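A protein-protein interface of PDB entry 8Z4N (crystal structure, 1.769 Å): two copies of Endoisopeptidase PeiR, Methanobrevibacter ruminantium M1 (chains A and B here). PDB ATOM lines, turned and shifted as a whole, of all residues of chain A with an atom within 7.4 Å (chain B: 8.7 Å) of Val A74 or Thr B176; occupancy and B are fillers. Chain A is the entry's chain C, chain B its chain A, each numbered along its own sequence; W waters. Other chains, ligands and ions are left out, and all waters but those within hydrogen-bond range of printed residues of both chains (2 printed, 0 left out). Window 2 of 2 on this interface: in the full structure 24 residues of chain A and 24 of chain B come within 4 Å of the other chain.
The side-chain amide nitrogen (ND2) of Asn B166 lies close to the side-chain amide nitrogen (ND2) of Asn B178 (3.1 Å). The backbone carbonyl oxygen (O) of Lys A46 is in hydrogen-bond range of the backbone NH (N) of Ala A75, at 3.0 Å. The backbone carbonyl oxygen of Gly A50 sits at hydrogen-bond distance from the side-chain hydroxyl of Ser A73, at 3.5 Å. The backbone carbonyl oxygen (O) of Thr B176 sits at hydrogen-bond distance from the guanidinium group (NH1) of Arg B169, 3.4 Å away. OD1 of Asp B174 is in salt-bridge range of NH2 of Arg B204, at 2.8 Å. The backbone carbonyl oxygen (O) of Ser B168 is in hydrogen-bond range of the backbone NH (N) of Gly B173 (3.0 Å).
Water W1 lies within hydrogen-bond range of OG1 of Thr B176, O of Leu A71 and N of Gly B177. Water W2 bridges O of Lys B200 (3.1 Å) and OE2 of Glu A53 (3.2 Å).
Hydrophobic or aromatic side chains of chain B that line the printed part of chain A: Tyr B175. Among the printed residues, Asp or Glu carboxylates within 4 Å of a Lys or Arg side-chain nitrogen of the other chain: Glu A53 with Lys B200.
Among the printed residues, merely in contact across the chains: Met A1 with Asn B178 (3.2 Å), Ser A73 with Asp B174 (3.3 Å), Thr A72 with Tyr B175 (3.4 Å), Val A74 with Gly B173 (3.4 Å), Ser A73 with Thr B176 (3.6 Å), Ala A75 with Lys B200 (3.6 Å), Val A74 with Thr B176 (3.9 Å) and Met A1 with Gly B177 (3.97 Å).
The side-chain amino group (NZ) of Lys B200 is in hydrogen-bond range of the backbone carbonyl oxygen (O) of Val A74 (2.8 Å). The side-chain carboxylate (OE1) of Glu A53 is in salt-bridge range of the side-chain amino group (NZ) of Lys B200 (3.0 Å). The backbone NH of Thr B176 lies within hydrogen-bond range of the backbone carbonyl oxygen of Thr A72. O of Thr A72 is in hydrogen-bond range of N of Gly B177, at 3.2 Å. O of Asp B174 lies within hydrogen-bond range of N of Val A74.
No position is printed for both chains. Of the 13 pairs that touch across the chains among the printed residues, none has its exchanged pair printed and touching as well.
Of chain B, only Gly B173 (3.4 Å), Asp B174 (3.1 Å), Thr B176 (3.9 Å) and Lys B200 (2.8 Å) come within 4 Å of Val A74. Thr B176 touches just these residues of chain A: Thr A72 (2.8 Å), Ser A73 (3.6 Å) and Val A74 (3.9 Å). Of the printed residues of chain B, Ser A73 touches Asp B174 and Thr B176. Of the printed residues of chain B, Met A1 touches Gly B177 and Asn B178. Of the printed residues of chain A, Tyr B175 touches Thr A72. Printed residues of chain A within 4 Å of Asn B178: Met A1. Of the printed residues of chain A, Asp B174 touches Ser A73 (3.3 Å) and Val A74 (3.1 Å).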
ATOM      1  N   MET A   1     -12.004  14.774 -14.354  1.00  0.00           N
ATOM      2  CA  MET A   1     -12.067  13.529 -13.588  1.00  0.00           C
ATOM      3  C   MET A   1     -12.693  13.738 -12.199  1.00  0.00           C
ATOM      4  O   MET A   1     -12.974  14.871 -11.780  1.00  0.00           O
ATOM      5  CB  MET A   1     -10.671  12.888 -13.461  1.00  0.00           C
ATOM      6  CG  MET A   1     -10.220  12.124 -14.724  1.00  0.00           C
ATOM      7  SD  MET A   1      -8.588  11.333 -14.637  1.00  0.00           S
ATOM      8  CE  MET A   1      -7.969  11.843 -16.248  1.00  0.00           C
ATOM      9  N   VAL A  44     -19.546   1.146  -8.952  1.00  0.00           N
ATOM     10  CA  VAL A  44     -19.724  -0.300  -9.061  1.00  0.00           C
ATOM     11  C   VAL A  44     -18.512  -0.940  -8.394  1.00  0.00           C
ATOM     12  O   VAL A  44     -17.537  -0.230  -8.113  1.00  0.00           O
ATOM     13  CB  VAL A  44     -19.898  -0.734 -10.525  1.00  0.00           C
ATOM     14  CG1 VAL A  44     -21.110  -0.016 -11.159  1.00  0.00           C
ATOM     15  CG2 VAL A  44     -18.659  -0.431 -11.324  1.00  0.00           C
ATOM     16  N   PRO A  45     -18.545  -2.241  -8.067  1.00  0.00           N
ATOM     17  CA  PRO A  45     -17.440  -2.839  -7.283  1.00  0.00           C
ATOM     18  C   PRO A  45     -16.053  -2.670  -7.884  1.00  0.00           C
ATOM     19  O   PRO A  45     -15.106  -2.439  -7.120  1.00  0.00           O
ATOM     20  CB  PRO A  45     -17.846  -4.316  -7.185  1.00  0.00           C
ATOM     21  CG  PRO A  45     -19.400  -4.234  -7.167  1.00  0.00           C
ATOM     22  CD  PRO A  45     -19.703  -3.158  -8.180  1.00  0.00           C
ATOM     23  N   LYS A  46     -15.879  -2.818  -9.205  1.00  0.00           N
ATOM     24  CA  LYS A  46     -14.541  -2.609  -9.773  1.00  0.00           C
ATOM     25  C   LYS A  46     -14.073  -1.173  -9.558  1.00  0.00           C
ATOM     26  O   LYS A  46     -12.859  -0.924  -9.454  1.00  0.00           O
ATOM     27  CB  LYS A  46     -14.514  -2.949 -11.265  1.00  0.00           C
ATOM     28  CG  LYS A  46     -15.272  -1.908 -12.091  1.00  0.00           C
ATOM     29  CD  LYS A  46     -15.204  -2.085 -13.600  1.00  0.00           C
ATOM     30  CE  LYS A  46     -15.025  -3.523 -14.055  1.00  0.00           C
ATOM     31  NZ  LYS A  46     -15.462  -3.627 -15.526  1.00  0.00           N
ATOM     32  N   GLU A  47     -15.015  -0.225  -9.456  1.00  0.00           N
ATOM     33  CA  GLU A  47     -14.664   1.175  -9.253  1.00  0.00           C
ATOM     34  C   GLU A  47     -14.331   1.475  -7.803  1.00  0.00           C
ATOM     35  O   GLU A  47     -13.356   2.172  -7.533  1.00  0.00           O
ATOM     36  CB  GLU A  47     -15.782   2.117  -9.721  1.00  0.00           C
ATOM     37  CG  GLU A  47     -16.054   2.072 -11.215  1.00  0.00           C
ATOM     38  CD  GLU A  47     -17.211   2.961 -11.631  1.00  0.00           C
ATOM     39  OE1 GLU A  47     -18.233   3.008 -10.910  1.00  0.00           O
ATOM     40  OE2 GLU A  47     -17.108   3.562 -12.716  1.00  0.00           O
ATOM     41  N   TYR A  48     -15.140   1.014  -6.845  1.00  0.00           N
ATOM     42  CA  TYR A  48     -14.743   1.332  -5.482  1.00  0.00           C
ATOM     43  C   TYR A  48     -13.519   0.523  -5.071  1.00  0.00           C
ATOM     44  O   TYR A  48     -12.696   1.008  -4.301  1.00  0.00           O
ATOM     45  CB  TYR A  48     -15.900   1.171  -4.499  1.00  0.00           C
ATOM     46  CG  TYR A  48     -16.546  -0.181  -4.277  1.00  0.00           C
ATOM     47  CD1 TYR A  48     -15.863  -1.214  -3.663  1.00  0.00           C
ATOM     48  CD2 TYR A  48     -17.901  -0.384  -4.605  1.00  0.00           C
ATOM     49  CE1 TYR A  48     -16.491  -2.442  -3.409  1.00  0.00           C
ATOM     50  CE2 TYR A  48     -18.551  -1.601  -4.339  1.00  0.00           C
ATOM     51  CZ  TYR A  48     -17.842  -2.629  -3.750  1.00  0.00           C
ATOM     52  OH  TYR A  48     -18.453  -3.845  -3.479  1.00  0.00           O
ATOM     53  N   ALA A  49     -13.359  -0.688  -5.600  1.00  0.00           N
ATOM     54  CA  ALA A  49     -12.133  -1.428  -5.336  1.00  0.00           C
ATOM     55  C   ALA A  49     -10.915  -0.701  -5.910  1.00  0.00           C
ATOM     56  O   ALA A  49      -9.853  -0.643  -5.274  1.00  0.00           O
ATOM     57  CB  ALA A  49     -12.247  -2.850  -5.910  1.00  0.00           C
ATOM     58  N   GLY A  50     -11.048  -0.159  -7.122  1.00  0.00           N
ATOM     59  CA  GLY A  50      -9.957   0.600  -7.720  1.00  0.00           C
ATOM     60  C   GLY A  50      -9.639   1.870  -6.958  1.00  0.00           C
ATOM     61  O   GLY A  50      -8.465   2.205  -6.759  1.00  0.00           O
ATOM     62  N   LEU A  51     -10.685   2.590  -6.515  1.00  0.00           N
ATOM     63  CA  LEU A  51     -10.494   3.813  -5.731  1.00  0.00           C
ATOM     64  C   LEU A  51      -9.764   3.522  -4.418  1.00  0.00           C
ATOM     65  O   LEU A  51      -8.816   4.228  -4.042  1.00  0.00           O
ATOM     66  CB  LEU A  51     -11.856   4.450  -5.436  1.00  0.00           C
ATOM     67  CG  LEU A  51     -11.907   5.729  -4.608  1.00  0.00           C
ATOM     68  CD1 LEU A  51     -11.410   6.882  -5.453  1.00  0.00           C
ATOM     69  CD2 LEU A  51     -13.353   6.012  -4.215  1.00  0.00           C
ATOM     70  N   GLU A  53      -8.022   0.818  -3.683  1.00  0.00           N
ATOM     71  CA  GLU A  53      -6.670   0.352  -3.972  1.00  0.00           C
ATOM     72  C   GLU A  53      -5.721   1.526  -4.106  1.00  0.00           C
ATOM     73  O   GLU A  53      -4.610   1.497  -3.568  1.00  0.00           O
ATOM     74  CB  GLU A  53      -6.652  -0.502  -5.233  1.00  0.00           C
ATOM     75  CG  GLU A  53      -5.295  -1.110  -5.551  1.00  0.00           C
ATOM     76  CD  GLU A  53      -5.298  -1.733  -6.926  1.00  0.00           C
ATOM     77  OE1 GLU A  53      -5.551  -1.011  -7.921  1.00  0.00           O
ATOM     78  OE2 GLU A  53      -5.124  -2.961  -7.010  1.00  0.00           O
ATOM     79  N   LEU A  71     -10.503   9.099  -8.975  1.00  0.00           N
ATOM     80  CA  LEU A  71     -10.887   7.812  -9.564  1.00  0.00           C
ATOM     81  C   LEU A  71     -10.198   7.641 -10.917  1.00  0.00           C
ATOM     82  O   LEU A  71     -10.584   8.296 -11.884  1.00  0.00           O
ATOM     83  CB  LEU A  71     -12.404   7.752  -9.736  1.00  0.00           C
ATOM     84  CG  LEU A  71     -13.024   6.454 -10.276  1.00  0.00           C
ATOM     85  CD1 LEU A  71     -12.460   5.210  -9.584  1.00  0.00           C
ATOM     86  CD2 LEU A  71     -14.546   6.478 -10.267  1.00  0.00           C
ATOM     87  N   THR A  72      -9.169   6.782 -10.996  1.00  0.00           N
ATOM     88  CA  THR A  72      -8.400   6.597 -12.228  1.00  0.00           C
ATOM     89  C   THR A  72      -8.348   5.159 -12.738  1.00  0.00           C
ATOM     90  O   THR A  72      -7.835   4.925 -13.845  1.00  0.00           O
ATOM     91  CB  THR A  72      -6.957   7.100 -12.044  1.00  0.00           C
ATOM     92  OG1 THR A  72      -6.313   6.390 -10.978  1.00  0.00           O
ATOM     93  CG2 THR A  72      -6.965   8.579 -11.721  1.00  0.00           C
ATOM     94  N   SER A  73      -8.820   4.194 -11.960  1.00  0.00           N
ATOM     95  CA  SER A  73      -8.507   2.799 -12.200  1.00  0.00           C
ATOM     96  C   SER A  73      -9.680   1.951 -11.743  1.00  0.00           C
ATOM     97  O   SER A  73     -10.651   2.454 -11.169  1.00  0.00           O
ATOM     98  CB  SER A  73      -7.240   2.402 -11.439  1.00  0.00           C
ATOM     99  OG  SER A  73      -7.451   2.637 -10.047  1.00  0.00           O
ATOM    100  N   VAL A  74      -9.620   0.668 -12.090  1.00  0.00           N
ATOM    101  CA  VAL A  74     -10.507  -0.356 -11.553  1.00  0.00           C
ATOM    102  C   VAL A  74      -9.643  -1.482 -10.982  1.00  0.00           C
ATOM    103  O   VAL A  74      -8.472  -1.631 -11.330  1.00  0.00           O
ATOM    104  CB  VAL A  74     -11.482  -0.884 -12.624  1.00  0.00           C
ATOM    105  CG1 VAL A  74     -12.294   0.274 -13.247  1.00  0.00           C
ATOM    106  CG2 VAL A  74     -10.687  -1.560 -13.710  1.00  0.00           C
ATOM    107  N   ALA A  75     -10.231  -2.289 -10.099  1.00  0.00           N
ATOM    108  CA  ALA A  75      -9.502  -3.413  -9.517  1.00  0.00           C
ATOM    109  C   ALA A  75     -10.504  -4.443  -9.031  1.00  0.00           C
ATOM    110  O   ALA A  75     -11.693  -4.156  -8.898  1.00  0.00           O
ATOM    111  CB  ALA A  75      -8.594  -2.987  -8.354  1.00  0.00           C
ATOM    112  N   ARG A  76     -10.005  -5.657  -8.793  1.00  0.00           N
ATOM    113  CA  ARG A  76     -10.811  -6.759  -8.288  1.00  0.00           C
ATOM    114  C   ARG A  76     -11.022  -6.692  -6.784  1.00  0.00           C
ATOM    115  O   ARG A  76     -11.922  -7.361  -6.274  1.00  0.00           O
ATOM    116  CB  ARG A  76     -10.181  -8.115  -8.629  1.00  0.00           C
ATOM    117  CG  ARG A  76      -9.890  -8.372 -10.097  1.00  0.00           C
ATOM    118  CD  ARG A  76      -9.011  -9.646 -10.222  1.00  0.00           C
ATOM    119  NE  ARG A  76      -9.410 -10.657  -9.243  1.00  0.00           N
ATOM    120  CZ  ARG A  76      -8.580 -11.425  -8.541  1.00  0.00           C
ATOM    121  NH1 ARG A  76      -7.265 -11.353  -8.693  1.00  0.00           N
ATOM    122  NH2 ARG A  76      -9.085 -12.288  -7.660  1.00  0.00           N
ATOM    123  N   ASN A  77     -10.144  -5.994  -6.074  1.00  0.00           N
ATOM    124  CA  ASN A  77     -10.234  -5.801  -4.637  1.00  0.00           C
ATOM    125  C   ASN A  77      -9.296  -4.658  -4.293  1.00  0.00           C
ATOM    126  O   ASN A  77      -8.530  -4.197  -5.156  1.00  0.00           O
ATOM    127  CB  ASN A  77      -9.880  -7.089  -3.873  1.00  0.00           C
ATOM    128  CG  ASN A  77      -8.450  -7.553  -4.153  1.00  0.00           C
ATOM    129  OD1 ASN A  77      -7.498  -6.779  -4.034  1.00  0.00           O
ATOM    130  ND2 ASN A  77      -8.307  -8.797  -4.556  1.00  0.00           N
ATOM    131  N   VAL B 165      -2.306   5.510 -20.654  1.00  0.00           N
ATOM    132  CA  VAL B 165      -3.159   4.447 -20.132  1.00  0.00           C
ATOM    133  C   VAL B 165      -4.534   4.445 -20.806  1.00  0.00           C
ATOM    134  O   VAL B 165      -5.156   3.388 -20.939  1.00  0.00           O
ATOM    135  CB  VAL B 165      -3.268   4.534 -18.597  1.00  0.00           C
ATOM    136  CG1 VAL B 165      -1.888   4.321 -17.988  1.00  0.00           C
ATOM    137  CG2 VAL B 165      -3.920   5.869 -18.126  1.00  0.00           C
ATOM    138  N   ASN B 166      -5.019   5.601 -21.264  1.00  0.00           N
ATOM    139  CA  ASN B 166      -6.313   5.618 -21.962  1.00  0.00           C
ATOM    140  C   ASN B 166      -6.288   4.805 -23.244  1.00  0.00           C
ATOM    141  O   ASN B 166      -7.314   4.240 -23.635  1.00  0.00           O
ATOM    142  CB  ASN B 166      -6.731   7.044 -22.285  1.00  0.00           C
ATOM    143  CG  ASN B 166      -5.610   7.836 -22.874  1.00  0.00           C
ATOM    144  OD1 ASN B 166      -4.589   8.060 -22.200  1.00  0.00           O
ATOM    145  ND2 ASN B 166      -5.760   8.270 -24.111  1.00  0.00           N
ATOM    146  N   GLN B 167      -5.123   4.692 -23.886  1.00  0.00           N
ATOM    147  CA  GLN B 167      -5.021   3.912 -25.108  1.00  0.00           C
ATOM    148  C   GLN B 167      -4.998   2.410 -24.869  1.00  0.00           C
ATOM    149  O   GLN B 167      -5.102   1.655 -25.841  1.00  0.00           O
ATOM    150  CB  GLN B 167      -3.762   4.352 -25.864  1.00  0.00           C
ATOM    151  CG  GLN B 167      -3.799   5.846 -26.245  1.00  0.00           C
ATOM    152  CD  GLN B 167      -2.696   6.251 -27.203  1.00  0.00           C
ATOM    153  OE1 GLN B 167      -2.161   5.418 -27.941  1.00  0.00           O
ATOM    154  NE2 GLN B 167      -2.314   7.535 -27.167  1.00  0.00           N
ATOM    155  N   SER B 168      -4.903   1.950 -23.610  1.00  0.00           N
ATOM    156  CA  SER B 168      -4.916   0.525 -23.304  1.00  0.00           C
ATOM    157  C   SER B 168      -6.195   0.098 -22.600  1.00  0.00           C
ATOM    158  O   SER B 168      -6.282  -1.028 -22.100  1.00  0.00           O
ATOM    159  CB  SER B 168      -3.693   0.165 -22.447  1.00  0.00           C
ATOM    160  OG  SER B 168      -3.777   0.794 -21.174  1.00  0.00           O
ATOM    161  N   ARG B 169      -7.200   0.962 -22.579  1.00  0.00           N
ATOM    162  CA  ARG B 169      -8.376   0.677 -21.774  1.00  0.00           C
ATOM    163  C   ARG B 169      -9.224  -0.438 -22.381  1.00  0.00           C
ATOM    164  O   ARG B 169      -9.781  -1.250 -21.652  1.00  0.00           O
ATOM    165  CB  ARG B 169      -9.163   1.956 -21.533  1.00  0.00           C
ATOM    166  CG  ARG B 169     -10.594   1.706 -21.156  1.00  0.00           C
ATOM    167  CD  ARG B 169     -11.270   2.999 -20.832  1.00  0.00           C
ATOM    168  NE  ARG B 169     -12.556   2.706 -20.219  1.00  0.00           N
ATOM    169  CZ  ARG B 169     -13.245   3.558 -19.479  1.00  0.00           C
ATOM    170  NH1 ARG B 169     -12.848   4.810 -19.317  1.00  0.00           N
ATOM    171  NH2 ARG B 169     -14.392   3.162 -18.942  1.00  0.00           N
ATOM    172  N   LYS B 172      -6.584  -3.788 -22.295  1.00  0.00           N
ATOM    173  CA  LYS B 172      -6.122  -4.306 -21.006  1.00  0.00           C
ATOM    174  C   LYS B 172      -7.099  -3.865 -19.928  1.00  0.00           C
ATOM    175  O   LYS B 172      -7.694  -4.712 -19.252  1.00  0.00           O
ATOM    176  CB  LYS B 172      -4.697  -3.852 -20.665  1.00  0.00           C
ATOM    177  CG  LYS B 172      -4.389  -3.944 -19.150  1.00  0.00           C
ATOM    178  CD  LYS B 172      -3.701  -5.223 -18.843  1.00  0.00           C
ATOM    179  CE  LYS B 172      -4.006  -5.690 -17.414  1.00  0.00           C
ATOM    180  NZ  LYS B 172      -3.637  -7.101 -17.228  1.00  0.00           N
ATOM    181  N   GLY B 173      -7.269  -2.555 -19.758  1.00  0.00           N
ATOM    182  CA  GLY B 173      -8.332  -2.020 -18.910  1.00  0.00           C
ATOM    183  C   GLY B 173      -8.045  -1.798 -17.438  1.00  0.00           C
ATOM    184  O   GLY B 173      -8.992  -1.704 -16.647  1.00  0.00           O
ATOM    185  N   ASP B 174      -6.784  -1.651 -17.037  1.00  0.00           N
ATOM    186  CA  ASP B 174      -6.529  -1.329 -15.639  1.00  0.00           C
ATOM    187  C   ASP B 174      -7.008   0.079 -15.293  1.00  0.00           C
ATOM    188  O   ASP B 174      -7.299   0.359 -14.125  1.00  0.00           O
ATOM    189  CB  ASP B 174      -5.033  -1.437 -15.320  1.00  0.00           C
ATOM    190  CG  ASP B 174      -4.583  -2.848 -15.036  1.00  0.00           C
ATOM    191  OD1 ASP B 174      -5.432  -3.767 -14.985  1.00  0.00           O
ATOM    192  OD2 ASP B 174      -3.347  -3.037 -14.872  1.00  0.00           O
ATOM    193  N   TYR B 175      -7.052   0.988 -16.272  1.00  0.00           N
ATOM    194  CA  TYR B 175      -7.255   2.408 -16.022  1.00  0.00           C
ATOM    195  C   TYR B 175      -8.457   2.956 -16.772  1.00  0.00           C
ATOM    196  O   TYR B 175      -8.701   2.586 -17.917  1.00  0.00           O
ATOM    197  CB  TYR B 175      -6.036   3.197 -16.453  1.00  0.00           C
ATOM    198  CG  TYR B 175      -4.785   2.831 -15.674  1.00  0.00           C
ATOM    199  CD1 TYR B 175      -4.545   3.402 -14.432  1.00  0.00           C
ATOM    200  CD2 TYR B 175      -3.870   1.917 -16.175  1.00  0.00           C
ATOM    201  CE1 TYR B 175      -3.411   3.085 -13.707  1.00  0.00           C
ATOM    202  CE2 TYR B 175      -2.730   1.574 -15.443  1.00  0.00           C
ATOM    203  CZ  TYR B 175      -2.514   2.162 -14.209  1.00  0.00           C
ATOM    204  OH  TYR B 175      -1.386   1.871 -13.475  1.00  0.00           O
ATOM    205  N   THR B 176      -9.176   3.877 -16.123  1.00  0.00           N
ATOM    206  CA  THR B 176     -10.243   4.645 -16.741  1.00  0.00           C
ATOM    207  C   THR B 176      -9.823   6.079 -17.016  1.00  0.00           C
ATOM    208  O   THR B 176     -10.477   6.765 -17.804  1.00  0.00           O
ATOM    209  CB  THR B 176     -11.478   4.669 -15.824  1.00  0.00           C
ATOM    210  OG1 THR B 176     -11.071   5.145 -14.541  1.00  0.00           O
ATOM    211  CG2 THR B 176     -12.056   3.271 -15.658  1.00  0.00           C
ATOM    212  N   GLY B 177      -8.718   6.519 -16.424  1.00  0.00           N
ATOM    213  CA  GLY B 177      -8.237   7.873 -16.554  1.00  0.00           C
ATOM    214  C   GLY B 177      -7.459   8.103 -17.836  1.00  0.00           C
ATOM    215  O   GLY B 177      -7.400   7.261 -18.738  1.00  0.00           O
ATOM    216  N   ASN B 178      -6.931   9.325 -17.938  1.00  0.00           N
ATOM    217  CA  ASN B 178      -6.186   9.838 -19.092  1.00  0.00           C
ATOM    218  C   ASN B 178      -4.871  10.450 -18.603  1.00  0.00           C
ATOM    219  O   ASN B 178      -4.884  11.545 -18.025  1.00  0.00           O
ATOM    220  CB  ASN B 178      -7.032  10.876 -19.812  1.00  0.00           C
ATOM    221  CG  ASN B 178      -7.768  10.305 -20.985  1.00  0.00           C
ATOM    222  OD1 ASN B 178      -8.972  10.054 -20.913  1.00  0.00           O
ATOM    223  ND2 ASN B 178      -7.076  10.174 -22.105  1.00  0.00           N
ATOM    224  N   PHE B 179      -3.748   9.750 -18.814  1.00  0.00           N
ATOM    225  CA  PHE B 179      -2.437  10.282 -18.453  1.00  0.00           C
ATOM    226  C   PHE B 179      -1.362   9.379 -19.042  1.00  0.00           C
ATOM    227  O   PHE B 179      -1.626   8.211 -19.352  1.00  0.00           O
ATOM    228  CB  PHE B 179      -2.257  10.401 -16.921  1.00  0.00           C
ATOM    229  CG  PHE B 179      -2.603   9.144 -16.139  1.00  0.00           C
ATOM    230  CD1 PHE B 179      -1.633   8.177 -15.876  1.00  0.00           C
ATOM    231  CD2 PHE B 179      -3.884   8.948 -15.622  1.00  0.00           C
ATOM    232  CE1 PHE B 179      -1.940   7.022 -15.152  1.00  0.00           C
ATOM    233  CE2 PHE B 179      -4.188   7.788 -14.881  1.00  0.00           C
ATOM    234  CZ  PHE B 179      -3.208   6.836 -14.648  1.00  0.00           C
ATOM    235  N   ALA B 199       1.644   1.807 -10.113  1.00  0.00           N
ATOM    236  CA  ALA B 199       0.333   2.236  -9.664  1.00  0.00           C
ATOM    237  C   ALA B 199      -0.658   1.087  -9.540  1.00  0.00           C
ATOM    238  O   ALA B 199      -1.818   1.336  -9.193  1.00  0.00           O
ATOM    239  CB  ALA B 199      -0.225   3.302 -10.630  1.00  0.00           C
ATOM    240  N   LYS B 200      -0.227  -0.144  -9.807  1.00  0.00           N
ATOM    241  CA  LYS B 200      -1.215  -1.244  -9.812  1.00  0.00           C
ATOM    242  C   LYS B 200      -0.700  -2.562  -9.239  1.00  0.00           C
ATOM    243  O   LYS B 200      -1.425  -3.167  -8.505  1.00  0.00           O
ATOM    244  CB  LYS B 200      -1.703  -1.486 -11.239  1.00  0.00           C
ATOM    245  CG  LYS B 200      -2.776  -0.524 -11.711  1.00  0.00           C
ATOM    246  CD  LYS B 200      -4.071  -1.209 -11.942  1.00  0.00           C
ATOM    247  CE  LYS B 200      -5.079  -1.018 -10.849  1.00  0.00           C
ATOM    248  NZ  LYS B 200      -5.851  -2.251 -10.595  1.00  0.00           N
ATOM    249  N   ARG B 204       1.273  -7.015 -14.048  1.00  0.00           N
ATOM    250  CA  ARG B 204       0.239  -6.618 -15.009  1.00  0.00           C
ATOM    251  C   ARG B 204       0.592  -7.127 -16.415  1.00  0.00           C
ATOM    252  O   ARG B 204       1.622  -6.750 -16.986  1.00  0.00           O
ATOM    253  CB  ARG B 204       0.086  -5.097 -15.012  1.00  0.00           C
ATOM    254  CG  ARG B 204      -0.038  -4.460 -13.634  1.00  0.00           C
ATOM    255  CD  ARG B 204      -0.964  -5.245 -12.703  1.00  0.00           C
ATOM    256  NE  ARG B 204      -2.355  -5.108 -13.124  1.00  0.00           N
ATOM    257  CZ  ARG B 204      -3.378  -5.635 -12.466  1.00  0.00           C
ATOM    258  NH1 ARG B 204      -3.194  -6.344 -11.357  1.00  0.00           N
ATOM    259  NH2 ARG B 204      -4.615  -5.443 -12.924  1.00  0.00           N
HETATM  260  O   HOH W   1     -11.486   7.662 -14.620  1.00  0.00           O
HETATM  261  O   HOH W   2      -2.304  -3.386  -5.566  1.00  0.00           O
